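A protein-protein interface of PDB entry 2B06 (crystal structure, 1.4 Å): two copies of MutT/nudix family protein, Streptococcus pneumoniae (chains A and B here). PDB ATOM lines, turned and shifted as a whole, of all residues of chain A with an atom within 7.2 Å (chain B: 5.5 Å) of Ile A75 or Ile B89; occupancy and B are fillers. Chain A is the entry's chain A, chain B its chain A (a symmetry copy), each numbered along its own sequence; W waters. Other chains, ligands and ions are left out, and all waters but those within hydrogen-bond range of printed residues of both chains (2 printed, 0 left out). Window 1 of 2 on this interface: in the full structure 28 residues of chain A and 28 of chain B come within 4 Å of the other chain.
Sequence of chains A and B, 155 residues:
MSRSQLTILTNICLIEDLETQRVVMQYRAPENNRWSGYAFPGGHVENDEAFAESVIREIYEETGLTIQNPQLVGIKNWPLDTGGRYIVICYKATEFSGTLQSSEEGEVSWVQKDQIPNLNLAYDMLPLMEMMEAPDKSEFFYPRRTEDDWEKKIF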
ATOM      1  N   PHE A  51     -20.271   8.633 -24.672  1.00  0.00           N
ATOM      2  CA  PHE A  51     -19.424   7.485 -24.383  1.00  0.00           C
ATOM      3  C   PHE A  51     -19.912   6.230 -25.124  1.00  0.00           C
ATOM      4  O   PHE A  51     -19.104   5.502 -25.701  1.00  0.00           O
ATOM      5  CB  PHE A  51     -19.331   7.235 -22.875  1.00  0.00           C
ATOM      6  CG  PHE A  51     -18.547   8.281 -22.145  1.00  0.00           C
ATOM      7  CD1 PHE A  51     -17.209   8.495 -22.459  1.00  0.00           C
ATOM      8  CD2 PHE A  51     -19.114   9.016 -21.110  1.00  0.00           C
ATOM      9  CE1 PHE A  51     -16.464   9.461 -21.789  1.00  0.00           C
ATOM     10  CE2 PHE A  51     -18.369   9.993 -20.437  1.00  0.00           C
ATOM     11  CZ  PHE A  51     -17.045  10.203 -20.765  1.00  0.00           C
ATOM     12  N   LEU A  72     -22.322  -0.694 -19.713  1.00  0.00           N
ATOM     13  CA  LEU A  72     -21.240  -0.231 -18.839  1.00  0.00           C
ATOM     14  C   LEU A  72     -21.002  -1.262 -17.748  1.00  0.00           C
ATOM     15  O   LEU A  72     -21.928  -1.636 -17.026  1.00  0.00           O
ATOM     16  CB  LEU A  72     -21.579   1.123 -18.202  1.00  0.00           C
ATOM     17  CG  LEU A  72     -20.601   1.786 -17.229  1.00  0.00           C
ATOM     18  CD1 LEU A  72     -19.305   2.127 -17.933  1.00  0.00           C
ATOM     19  CD2 LEU A  72     -21.223   3.053 -16.655  1.00  0.00           C
ATOM     20  N   VAL A  73     -19.764  -1.731 -17.629  1.00  0.00           N
ATOM     21  CA  VAL A  73     -19.438  -2.745 -16.628  1.00  0.00           C
ATOM     22  C   VAL A  73     -18.336  -2.305 -15.671  1.00  0.00           C
ATOM     23  O   VAL A  73     -18.024  -3.018 -14.716  1.00  0.00           O
ATOM     24  CB  VAL A  73     -19.102  -4.116 -17.281  1.00  0.00           C
ATOM     25  CG1 VAL A  73     -20.352  -4.685 -17.965  1.00  0.00           C
ATOM     26  CG2 VAL A  73     -17.953  -3.977 -18.258  1.00  0.00           C
ATOM     27  N   GLY A  74     -17.732  -1.150 -15.930  1.00  0.00           N
ATOM     28  CA  GLY A  74     -16.743  -0.619 -15.007  1.00  0.00           C
ATOM     29  C   GLY A  74     -15.859   0.449 -15.604  1.00  0.00           C
ATOM     30  O   GLY A  74     -16.016   0.843 -16.767  1.00  0.00           O
ATOM     31  N   ILE A  75     -14.963   0.951 -14.767  1.00  0.00           N
ATOM     32  CA  ILE A  75     -14.045   1.992 -15.176  1.00  0.00           C
ATOM     33  C   ILE A  75     -12.656   1.603 -14.710  1.00  0.00           C
ATOM     34  O   ILE A  75     -12.460   1.296 -13.528  1.00  0.00           O
ATOM     35  CB  ILE A  75     -14.430   3.357 -14.553  1.00  0.00           C
ATOM     36  CG1 ILE A  75     -15.805   3.818 -15.043  1.00  0.00           C
ATOM     37  CG2 ILE A  75     -13.391   4.402 -14.919  1.00  0.00           C
ATOM     38  CD1 ILE A  75     -16.322   5.066 -14.351  1.00  0.00           C
ATOM     39  N   LYS A  76     -11.700   1.589 -15.634  1.00  0.00           N
ATOM     40  CA  LYS A  76     -10.294   1.410 -15.271  1.00  0.00           C
ATOM     41  C   LYS A  76      -9.620   2.781 -15.339  1.00  0.00           C
ATOM     42  O   LYS A  76      -9.797   3.520 -16.307  1.00  0.00           O
ATOM     43  CB  LYS A  76      -9.610   0.413 -16.220  1.00  0.00           C
ATOM     44  CG  LYS A  76      -8.126   0.197 -15.951  1.00  0.00           C
ATOM     45  CD  LYS A  76      -7.504  -0.663 -17.049  1.00  0.00           C
ATOM     46  CE  LYS A  76      -6.061  -0.993 -16.711  1.00  0.00           C
ATOM     47  NZ  LYS A  76      -5.360  -1.614 -17.882  1.00  0.00           N
ATOM     48  N   ASN A  77      -8.879   3.164 -14.310  1.00  0.00           N
ATOM     49  CA  ASN A  77      -8.291   4.481 -14.346  1.00  0.00           C
ATOM     50  C   ASN A  77      -7.080   4.610 -13.447  1.00  0.00           C
ATOM     51  O   ASN A  77      -6.878   3.805 -12.534  1.00  0.00           O
ATOM     52  CB  ASN A  77      -9.345   5.547 -13.992  1.00  0.00           C
ATOM     53  CG  ASN A  77      -9.732   5.533 -12.524  1.00  0.00           C
ATOM     54  OD1 ASN A  77     -10.358   4.587 -12.023  1.00  0.00           O
ATOM     55  ND2 ASN A  77      -9.393   6.588 -11.836  1.00  0.00           N
ATOM     56  N   TYR A  86      -5.835   8.955 -16.552  1.00  0.00           N
ATOM     57  CA  TYR A  86      -6.167   8.122 -17.696  1.00  0.00           C
ATOM     58  C   TYR A  86      -7.419   7.340 -17.345  1.00  0.00           C
ATOM     59  O   TYR A  86      -7.491   6.701 -16.293  1.00  0.00           O
ATOM     60  CB  TYR A  86      -5.015   7.159 -18.005  1.00  0.00           C
ATOM     61  CG  TYR A  86      -4.959   6.749 -19.455  1.00  0.00           C
ATOM     62  CD1 TYR A  86      -4.060   7.362 -20.321  1.00  0.00           C
ATOM     63  CD2 TYR A  86      -5.823   5.785 -19.968  1.00  0.00           C
ATOM     64  CE1 TYR A  86      -4.006   7.014 -21.660  1.00  0.00           C
ATOM     65  CE2 TYR A  86      -5.769   5.423 -21.324  1.00  0.00           C
ATOM     66  CZ  TYR A  86      -4.858   6.054 -22.146  1.00  0.00           C
ATOM     67  OH  TYR A  86      -4.776   5.741 -23.483  1.00  0.00           O
ATOM     68  N   ILE A  87      -8.421   7.421 -18.219  1.00  0.00           N
ATOM     69  CA  ILE A  87      -9.717   6.813 -17.970  1.00  0.00           C
ATOM     70  C   ILE A  87     -10.084   5.864 -19.102  1.00  0.00           C
ATOM     71  O   ILE A  87     -10.003   6.214 -20.285  1.00  0.00           O
ATOM     72  CB  ILE A  87     -10.811   7.884 -17.830  1.00  0.00           C
ATOM     73  CG1 ILE A  87     -10.504   8.804 -16.641  1.00  0.00           C
ATOM     74  CG2 ILE A  87     -12.190   7.228 -17.650  1.00  0.00           C
ATOM     75  CD1 ILE A  87     -11.449   9.990 -16.540  1.00  0.00           C
ATOM     76  N   VAL A  88     -10.454   4.646 -18.721  1.00  0.00           N
ATOM     77  CA  VAL A  88     -10.969   3.629 -19.643  1.00  0.00           C
ATOM     78  C   VAL A  88     -12.384   3.225 -19.235  1.00  0.00           C
ATOM     79  O   VAL A  88     -12.573   2.606 -18.194  1.00  0.00           O
ATOM     80  CB  VAL A  88     -10.089   2.376 -19.673  1.00  0.00           C
ATOM     81  CG1 VAL A  88     -10.505   1.514 -20.871  1.00  0.00           C
ATOM     82  CG2 VAL A  88      -8.621   2.754 -19.785  1.00  0.00           C
ATOM     83  N   ILE A  89     -13.374   3.588 -20.042  1.00  0.00           N
ATOM     84  CA  ILE A  89     -14.750   3.185 -19.776  1.00  0.00           C
ATOM     85  C   ILE A  89     -14.920   1.792 -20.360  1.00  0.00           C
ATOM     86  O   ILE A  89     -14.667   1.588 -21.546  1.00  0.00           O
ATOM     87  CB  ILE A  89     -15.759   4.181 -20.382  1.00  0.00           C
ATOM     88  CG1 ILE A  89     -15.393   5.631 -20.004  1.00  0.00           C
ATOM     89  CG2 ILE A  89     -17.190   3.818 -19.989  1.00  0.00           C
ATOM     90  CD1 ILE A  89     -15.463   5.939 -18.511  1.00  0.00           C
ATOM     91  N   CYS A  90     -15.314   0.847 -19.519  1.00  0.00           N
ATOM     92  CA  CYS A  90     -15.349  -0.568 -19.898  1.00  0.00           C
ATOM     93  C   CYS A  90     -16.750  -1.040 -20.185  1.00  0.00           C
ATOM     94  O   CYS A  90     -17.647  -0.865 -19.353  1.00  0.00           O
ATOM     95  CB  CYS A  90     -14.758  -1.430 -18.780  1.00  0.00           C
ATOM     96  SG  CYS A  90     -13.056  -1.000 -18.315  1.00  0.00           S
ATOM     97  N   LEU A 128      -8.634  -7.382 -14.793  1.00  0.00           N
ATOM     98  CA  LEU A 128      -9.523  -6.400 -15.432  1.00  0.00           C
ATOM     99  C   LEU A 128     -10.794  -7.083 -15.924  1.00  0.00           C
ATOM    100  O   LEU A 128     -11.906  -6.613 -15.660  1.00  0.00           O
ATOM    101  CB  LEU A 128      -8.820  -5.686 -16.592  1.00  0.00           C
ATOM    102  CG  LEU A 128      -9.696  -4.774 -17.465  1.00  0.00           C
ATOM    103  CD1 LEU A 128     -10.289  -3.614 -16.661  1.00  0.00           C
ATOM    104  CD2 LEU A 128      -8.888  -4.235 -18.634  1.00  0.00           C
ATOM    105  N   MET A 131     -12.951  -7.917 -12.954  1.00  0.00           N
ATOM    106  CA  MET A 131     -13.682  -6.744 -12.452  1.00  0.00           C
ATOM    107  C   MET A 131     -14.895  -6.465 -13.338  1.00  0.00           C
ATOM    108  O   MET A 131     -15.998  -6.199 -12.844  1.00  0.00           O
ATOM    109  CB  MET A 131     -12.783  -5.503 -12.379  1.00  0.00           C
ATOM    110  CG  MET A 131     -13.526  -4.185 -11.957  1.00  0.00           C
ATOM    111  SD  MET A 131     -14.484  -3.310 -13.292  1.00  0.00           S
ATOM    112  CE  MET A 131     -13.135  -2.500 -14.123  1.00  0.00           C
ATOM    113  N   MET A 132     -14.695  -6.545 -14.647  1.00  0.00           N
ATOM    114  CA  MET A 132     -15.763  -6.232 -15.589  1.00  0.00           C
ATOM    115  C   MET A 132     -16.912  -7.223 -15.425  1.00  0.00           C
ATOM    116  O   MET A 132     -18.065  -6.811 -15.315  1.00  0.00           O
ATOM    117  CB  MET A 132     -15.224  -6.226 -17.024  1.00  0.00           C
ATOM    118  CG  MET A 132     -14.253  -5.067 -17.325  1.00  0.00           C
ATOM    119  SD  MET A 132     -13.370  -5.164 -18.948  1.00  0.00           S
ATOM    120  CE  MET A 132     -14.738  -5.128 -20.167  1.00  0.00           C
ATOM    121  N   LYS A 137     -18.608  -5.270  -8.833  1.00  0.00           N
ATOM    122  CA  LYS A 137     -17.372  -4.493  -8.914  1.00  0.00           C
ATOM    123  C   LYS A 137     -17.433  -3.614 -10.135  1.00  0.00           C
ATOM    124  O   LYS A 137     -17.914  -4.040 -11.192  1.00  0.00           O
ATOM    125  CB  LYS A 137     -16.140  -5.399  -9.008  1.00  0.00           C
ATOM    126  CG  LYS A 137     -15.975  -6.407  -7.867  1.00  0.00           C
ATOM    127  CD  LYS A 137     -15.745  -5.726  -6.519  1.00  0.00           C
ATOM    128  CE  LYS A 137     -15.736  -6.768  -5.411  1.00  0.00           C
ATOM    129  NZ  LYS A 137     -15.528  -6.165  -4.076  1.00  0.00           N
ATOM    130  N   SER A 138     -16.911  -2.400 -10.016  1.00  0.00           N
ATOM    131  CA  SER A 138     -17.002  -1.445 -11.109  1.00  0.00           C
ATOM    132  C   SER A 138     -15.806  -0.528 -11.313  1.00  0.00           C
ATOM    133  O   SER A 138     -15.859   0.341 -12.197  1.00  0.00           O
ATOM    134  CB  SER A 138     -18.274  -0.600 -11.009  1.00  0.00           C
ATOM    135  OG  SER A 138     -18.427  -0.042  -9.726  1.00  0.00           O
ATOM    136  N   GLU A 139     -14.741  -0.698 -10.534  1.00  0.00           N
ATOM    137  CA  GLU A 139     -13.584   0.151 -10.741  1.00  0.00           C
ATOM    138  C   GLU A 139     -12.303  -0.631 -10.542  1.00  0.00           C
ATOM    139  O   GLU A 139     -12.172  -1.427  -9.608  1.00  0.00           O
ATOM    140  CB  GLU A 139     -13.611   1.395  -9.831  1.00  0.00           C
ATOM    141  CG  GLU A 139     -12.442   2.378 -10.095  1.00  0.00           C
ATOM    142  CD  GLU A 139     -12.458   3.621  -9.225  1.00  0.00           C
ATOM    143  OE1 GLU A 139     -13.341   3.717  -8.337  1.00  0.00           O
ATOM    144  OE2 GLU A 139     -11.554   4.474  -9.441  1.00  0.00           O
ATOM    145  N   PHE A 140     -11.376  -0.394 -11.457  1.00  0.00           N
ATOM    146  CA  PHE A 140     -10.026  -0.918 -11.393  1.00  0.00           C
ATOM    147  C   PHE A 140      -9.135   0.316 -11.348  1.00  0.00           C
ATOM    148  O   PHE A 140      -9.111   1.102 -12.306  1.00  0.00           O
ATOM    149  CB  PHE A 140      -9.763  -1.763 -12.654  1.00  0.00           C
ATOM    150  CG  PHE A 140      -8.423  -2.448 -12.672  1.00  0.00           C
ATOM    151  CD1 PHE A 140      -8.340  -3.830 -12.741  1.00  0.00           C
ATOM    152  CD2 PHE A 140      -7.241  -1.702 -12.637  1.00  0.00           C
ATOM    153  CE1 PHE A 140      -7.093  -4.469 -12.760  1.00  0.00           C
ATOM    154  CE2 PHE A 140      -6.001  -2.330 -12.662  1.00  0.00           C
ATOM    155  CZ  PHE A 140      -5.932  -3.711 -12.723  1.00  0.00           C
ATOM    156  N   PHE A 141      -8.435   0.510 -10.238  1.00  0.00           N
ATOM    157  CA  PHE A 141      -7.686   1.739 -10.022  1.00  0.00           C
ATOM    158  C   PHE A 141      -6.237   1.436  -9.690  1.00  0.00           C
ATOM    159  O   PHE A 141      -5.971   0.571  -8.864  1.00  0.00           O
ATOM    160  CB  PHE A 141      -8.341   2.489  -8.857  1.00  0.00           C
ATOM    161  CG  PHE A 141      -7.657   3.758  -8.460  1.00  0.00           C
ATOM    162  CD1 PHE A 141      -7.667   4.875  -9.283  1.00  0.00           C
ATOM    163  CD2 PHE A 141      -7.050   3.865  -7.212  1.00  0.00           C
ATOM    164  CE1 PHE A 141      -7.067   6.070  -8.890  1.00  0.00           C
ATOM    165  CE2 PHE A 141      -6.454   5.064  -6.813  1.00  0.00           C
ATOM    166  CZ  PHE A 141      -6.458   6.159  -7.648  1.00  0.00           C
ATOM    167  N   LYS A 153      -6.279  -1.554  -7.051  1.00  0.00           N
ATOM    168  CA  LYS A 153      -7.416  -1.645  -6.150  1.00  0.00           C
ATOM    169  C   LYS A 153      -8.635  -1.912  -7.020  1.00  0.00           C
ATOM    170  O   LYS A 153      -8.785  -1.315  -8.098  1.00  0.00           O
ATOM    171  CB  LYS A 153      -7.616  -0.324  -5.420  1.00  0.00           C
ATOM    172  CG  LYS A 153      -6.615  -0.067  -4.315  1.00  0.00           C
ATOM    173  CD  LYS A 153      -6.959   1.218  -3.566  1.00  0.00           C
ATOM    174  CE  LYS A 153      -6.659   1.120  -2.074  1.00  0.00           C
ATOM    175  NZ  LYS A 153      -5.418   0.378  -1.797  1.00  0.00           N
ATOM    176  N   PHE A 155     -12.777  -1.811  -6.774  1.00  0.00           N
ATOM    177  CA  PHE A 155     -13.939  -1.344  -6.006  1.00  0.00           C
ATOM    178  C   PHE A 155     -15.242  -1.775  -6.650  1.00  0.00           C
ATOM    179  O   PHE A 155     -15.287  -1.964  -7.861  1.00  0.00           O
ATOM    180  CB  PHE A 155     -13.950   0.183  -5.931  1.00  0.00           C
ATOM    181  CG  PHE A 155     -12.700   0.784  -5.363  1.00  0.00           C
ATOM    182  CD1 PHE A 155     -11.725   1.286  -6.206  1.00  0.00           C
ATOM    183  CD2 PHE A 155     -12.512   0.887  -3.994  1.00  0.00           C
ATOM    184  CE1 PHE A 155     -10.592   1.873  -5.696  1.00  0.00           C
ATOM    185  CE2 PHE A 155     -11.352   1.472  -3.487  1.00  0.00           C
ATOM    186  CZ  PHE A 155     -10.397   1.963  -4.346  1.00  0.00           C
ATOM    187  OXT PHE A 155     -16.282  -1.897  -5.982  1.00  0.00           O
ATOM    188  N   THR B  10     -16.771  14.587 -11.555  1.00  0.00           N
ATOM    189  CA  THR B  10     -17.618  14.681 -10.364  1.00  0.00           C
ATOM    190  C   THR B  10     -18.349  13.378 -10.132  1.00  0.00           C
ATOM    191  O   THR B  10     -18.349  12.483 -10.980  1.00  0.00           O
ATOM    192  CB  THR B  10     -18.681  15.814 -10.458  1.00  0.00           C
ATOM    193  OG1 THR B  10     -19.704  15.466 -11.411  1.00  0.00           O
ATOM    194  CG2 THR B  10     -18.045  17.173 -10.816  1.00  0.00           C
ATOM    195  N   ASN B  11     -18.988  13.273  -8.971  1.00  0.00           N
ATOM    196  CA  ASN B  11     -19.813  12.102  -8.666  1.00  0.00           C
ATOM    197  C   ASN B  11     -21.120  12.515  -8.000  1.00  0.00           C
ATOM    198  O   ASN B  11     -21.246  13.628  -7.485  1.00  0.00           O
ATOM    199  CB  ASN B  11     -19.047  11.102  -7.787  1.00  0.00           C
ATOM    200  CG  ASN B  11     -18.462  11.741  -6.562  1.00  0.00           C
ATOM    201  OD1 ASN B  11     -19.191  12.278  -5.728  1.00  0.00           O
ATOM    202  ND2 ASN B  11     -17.129  11.695  -6.442  1.00  0.00           N
ATOM    203  N   ILE B  12     -22.083  11.600  -8.032  1.00  0.00           N
ATOM    204  CA  ILE B  12     -23.278  11.707  -7.202  1.00  0.00           C
ATOM    205  C   ILE B  12     -23.586  10.338  -6.669  1.00  0.00           C
ATOM    206  O   ILE B  12     -23.149   9.322  -7.211  1.00  0.00           O
ATOM    207  CB  ILE B  12     -24.515  12.284  -7.940  1.00  0.00           C
ATOM    208  CG1 ILE B  12     -24.912  11.402  -9.131  1.00  0.00           C
ATOM    209  CG2 ILE B  12     -24.282  13.751  -8.337  1.00  0.00           C
ATOM    210  CD1 ILE B  12     -26.122  11.892  -9.884  1.00  0.00           C
ATOM    211  N   PHE B  51     -12.208   6.905  -8.080  1.00  0.00           N
ATOM    212  CA  PHE B  51     -13.588   7.357  -8.181  1.00  0.00           C
ATOM    213  C   PHE B  51     -14.421   6.888  -6.978  1.00  0.00           C
ATOM    214  O   PHE B  51     -15.187   7.671  -6.416  1.00  0.00           O
ATOM    215  CB  PHE B  51     -14.219   6.905  -9.502  1.00  0.00           C
ATOM    216  CG  PHE B  51     -13.663   7.608 -10.701  1.00  0.00           C
ATOM    217  CD1 PHE B  51     -13.780   8.989 -10.814  1.00  0.00           C
ATOM    218  CD2 PHE B  51     -13.075   6.901 -11.743  1.00  0.00           C
ATOM    219  CE1 PHE B  51     -13.271   9.660 -11.922  1.00  0.00           C
ATOM    220  CE2 PHE B  51     -12.557   7.573 -12.858  1.00  0.00           C
ATOM    221  CZ  PHE B  51     -12.670   8.945 -12.954  1.00  0.00           C
ATOM    222  N   LEU B  72     -21.451   1.486  -9.086  1.00  0.00           N
ATOM    223  CA  LEU B  72     -21.556   2.299 -10.302  1.00  0.00           C
ATOM    224  C   LEU B  72     -22.847   1.954 -11.024  1.00  0.00           C
ATOM    225  O   LEU B  72     -23.102   0.788 -11.333  1.00  0.00           O
ATOM    226  CB  LEU B  72     -20.363   2.059 -11.238  1.00  0.00           C
ATOM    227  CG  LEU B  72     -20.278   2.784 -12.583  1.00  0.00           C
ATOM    228  CD1 LEU B  72     -20.168   4.279 -12.371  1.00  0.00           C
ATOM    229  CD2 LEU B  72     -19.068   2.285 -13.362  1.00  0.00           C
ATOM    230  N   GLY B  74     -24.151   4.409 -13.530  1.00  0.00           N
ATOM    231  CA  GLY B  74     -24.179   5.134 -14.790  1.00  0.00           C
ATOM    232  C   GLY B  74     -23.302   6.364 -14.809  1.00  0.00           C
ATOM    233  O   GLY B  74     -22.605   6.675 -13.835  1.00  0.00           O
ATOM    234  N   ILE B  75     -23.309   7.024 -15.957  1.00  0.00           N
ATOM    235  CA  ILE B  75     -22.514   8.219 -16.147  1.00  0.00           C
ATOM    236  C   ILE B  75     -23.395   9.271 -16.791  1.00  0.00           C
ATOM    237  O   ILE B  75     -24.029   9.006 -17.820  1.00  0.00           O
ATOM    238  CB  ILE B  75     -21.296   7.943 -17.062  1.00  0.00           C
ATOM    239  CG1 ILE B  75     -20.347   6.926 -16.424  1.00  0.00           C
ATOM    240  CG2 ILE B  75     -20.544   9.235 -17.323  1.00  0.00           C
ATOM    241  CD1 ILE B  75     -19.213   6.482 -17.331  1.00  0.00           C
ATOM    242  N   LYS B  76     -23.459  10.450 -16.180  1.00  0.00           N
ATOM    243  CA  LYS B  76     -24.126  11.594 -16.801  1.00  0.00           C
ATOM    244  C   LYS B  76     -23.040  12.521 -17.349  1.00  0.00           C
ATOM    245  O   LYS B  76     -22.066  12.823 -16.660  1.00  0.00           O
ATOM    246  CB  LYS B  76     -25.012  12.327 -15.781  1.00  0.00           C
ATOM    247  CG  LYS B  76     -25.712  13.566 -16.325  1.00  0.00           C
ATOM    248  CD  LYS B  76     -26.417  14.319 -15.197  1.00  0.00           C
ATOM    249  CE  LYS B  76     -27.227  15.475 -15.757  1.00  0.00           C
ATOM    250  NZ  LYS B  76     -27.716  16.372 -14.660  1.00  0.00           N
ATOM    251  N   ILE B  87     -18.392  15.515 -16.515  1.00  0.00           N
ATOM    252  CA  ILE B  87     -18.636  14.112 -16.226  1.00  0.00           C
ATOM    253  C   ILE B  87     -19.126  13.944 -14.793  1.00  0.00           C
ATOM    254  O   ILE B  87     -18.533  14.473 -13.846  1.00  0.00           O
ATOM    255  CB  ILE B  87     -17.361  13.277 -16.428  1.00  0.00           C
ATOM    256  CG1 ILE B  87     -16.896  13.365 -17.888  1.00  0.00           C
ATOM    257  CG2 ILE B  87     -17.608  11.810 -16.039  1.00  0.00           C
ATOM    258  CD1 ILE B  87     -15.549  12.704 -18.129  1.00  0.00           C
ATOM    259  N   VAL B  88     -20.236  13.228 -14.657  1.00  0.00           N
ATOM    260  CA  VAL B  88     -20.796  12.841 -13.358  1.00  0.00           C
ATOM    261  C   VAL B  88     -20.857  11.319 -13.250  1.00  0.00           C
ATOM    262  O   VAL B  88     -21.631  10.680 -13.953  1.00  0.00           O
ATOM    263  CB  VAL B  88     -22.204  13.405 -13.143  1.00  0.00           C
ATOM    264  CG1 VAL B  88     -22.582  13.230 -11.667  1.00  0.00           C
ATOM    265  CG2 VAL B  88     -22.257  14.875 -13.527  1.00  0.00           C
ATOM    266  N   ILE B  89     -20.031  10.740 -12.385  1.00  0.00           N
ATOM    267  CA  ILE B  89     -20.068   9.300 -12.156  1.00  0.00           C
ATOM    268  C   ILE B  89     -21.160   9.045 -11.131  1.00  0.00           C
ATOM    269  O   ILE B  89     -21.128   9.620 -10.045  1.00  0.00           O
ATOM    270  CB  ILE B  89     -18.702   8.769 -11.676  1.00  0.00           C
ATOM    271  CG1 ILE B  89     -17.564   9.284 -12.580  1.00  0.00           C
ATOM    272  CG2 ILE B  89     -18.716   7.245 -11.563  1.00  0.00           C
ATOM    273  CD1 ILE B  89     -17.629   8.799 -14.026  1.00  0.00           C
ATOM    274  N   CYS B  90     -22.125   8.214 -11.496  1.00  0.00           N
ATOM    275  CA  CYS B  90     -23.328   8.013 -10.684  1.00  0.00           C
ATOM    276  C   CYS B  90     -23.284   6.715  -9.922  1.00  0.00           C
ATOM    277  O   CYS B  90     -23.066   5.653 -10.517  1.00  0.00           O
ATOM    278  CB  CYS B  90     -24.575   8.020 -11.573  1.00  0.00           C
ATOM    279  SG  CYS B  90     -24.791   9.531 -12.558  1.00  0.00           S
ATOM    280  N   TYR B  91     -23.520   6.807  -8.617  1.00  0.00           N
ATOM    281  CA  TYR B  91     -23.480   5.650  -7.729  1.00  0.00           C
ATOM    282  C   TYR B  91     -24.797   5.429  -7.016  1.00  0.00           C
ATOM    283  O   TYR B  91     -25.587   6.367  -6.864  1.00  0.00           O
ATOM    284  CB  TYR B  91     -22.408   5.840  -6.664  1.00  0.00           C
ATOM    285  CG  TYR B  91     -20.999   5.850  -7.213  1.00  0.00           C
ATOM    286  CD1 TYR B  91     -20.261   4.683  -7.290  1.00  0.00           C
ATOM    287  CD2 TYR B  91     -20.404   7.033  -7.638  1.00  0.00           C
ATOM    288  CE1 TYR B  91     -18.961   4.682  -7.776  1.00  0.00           C
ATOM    289  CE2 TYR B  91     -19.106   7.050  -8.121  1.00  0.00           C
ATOM    290  CZ  TYR B  91     -18.395   5.872  -8.169  1.00  0.00           C
ATOM    291  OH  TYR B  91     -17.114   5.875  -8.658  1.00  0.00           O
HETATM  292  O   HOH W   1     -20.496  -1.521  -8.923  1.00  0.00           O
HETATM  293  O   HOH W   2     -16.017   3.451  -8.748  1.00  0.00           O
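The backbone NH (N) of Phe B51 is in hydrogen-bond range of the side-chain carboxylate (OE2) of Glu A139. The side-chain hydroxyl (OG) of Ser A138 lies close to the backbone NH (N) of Leu B72, at 3.4 Å.
The backbone NH (N) of Phe A155 is in hydrogen-bond range of the backbone carbonyl oxygen (O) of Glu A139, 2.9 Å away. The side-chain carboxylate (OE2) of Glu A139 sits close to the side-chain amide oxygen (OD1) of Asn A77. The backbone carbonyl oxygen of Thr B10 is in hydrogen-bond range of the backbone NH of Ile B89 (2.8 Å). O of Phe A155 is in hydrogen-bond range of N of Ser A138. N of Asn A77 lies within hydrogen-bond range of O of Phe A140, at 2.9 Å. N of Ile B12 sits at hydrogen-bond distance from O of Ile B89, 3.0 Å away.
Among the printed residues, merely in contact across the chains: Asn A77 with Phe B51 (3.5 Å), Ile A75 with Phe B51 (3.9 Å), Phe A51 with Ile B75 (3.9 Å), Phe A51 with Ile B87 (3.9 Å), Ile A87 with Phe B51 (3.9 Å), Ile A75 with Ile B89 (3.97 Å), Ile A89 with Ile B75 (3.97 Å), Leu A72 with Ile B75 (3.98 Å) and Ile A75 with Leu B72 (3.98 Å).
Of the printed residues of chain B, Ile A75 touches Phe B51 (3.9 Å), Leu B72 (3.98 Å) and Ile B89 (3.97 Å). Of the printed residues of chain B, Asn A77 touches Phe B51. Of the printed residues of chain B, Glu A139 touches Phe B51. Of the printed residues of chain A, Leu B72 touches Ile A75 (3.98 Å) and Ser A138 (3.2 Å). Of the printed residues of chain A, Ile B75 touches Phe A51 (3.9 Å), Leu A72 (3.98 Å) and Ile A89 (3.97 Å). Of the printed residues of chain A, Ile B87 touches Phe A51. Ile B89 touches just one residue of chain A: Ile A75 (3.97 Å). The nearest residue of chain B that does not touch Ile A75 is Ile B75 (4.4 Å).
Hydrophobic or aromatic side chains of chain A within 4 Å of the printed part of chain B: Phe A51, Leu A72, Ile A75, Ile A87 and Ile A89. Of the 13 printed residues of chain B, 5 touch a printed residue of chain A. Among the printed residues, 11 pairs touch across the chains. Among the printed residues, no Asp or Glu carboxylate lies within 4 Å of a Lys or Arg side-chain nitrogen of the other chain.
Phe A51 touches Ile B75, and with the chains exchanged Ile A75 touches Phe B51. Phe A51 touches Ile B87, and with the chains exchanged Ile A87 touches Phe B51. Leu A72 touches Ile B75, and with the chains exchanged Ile A75 touches Leu B72. Ile A75 touches Ile B89, and with the chains exchanged Ile A89 touches Ile B75. Positions printed for both chains: 51, 72, 74, 75, 76, 87, 88, 89 and 90. Of the 11 pairs that touch across the chains among the printed residues, 8 have their exchanged pair printed and touching as well.
Water W2 lies within hydrogen-bond range of OH of Tyr B91 (2.7 Å) and OE1 of Glu A139 (2.7 Å). Water W1 lies within hydrogen-bond range of the side-chain hydroxyl of Ser A138 and the backbone NH of Leu B72.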
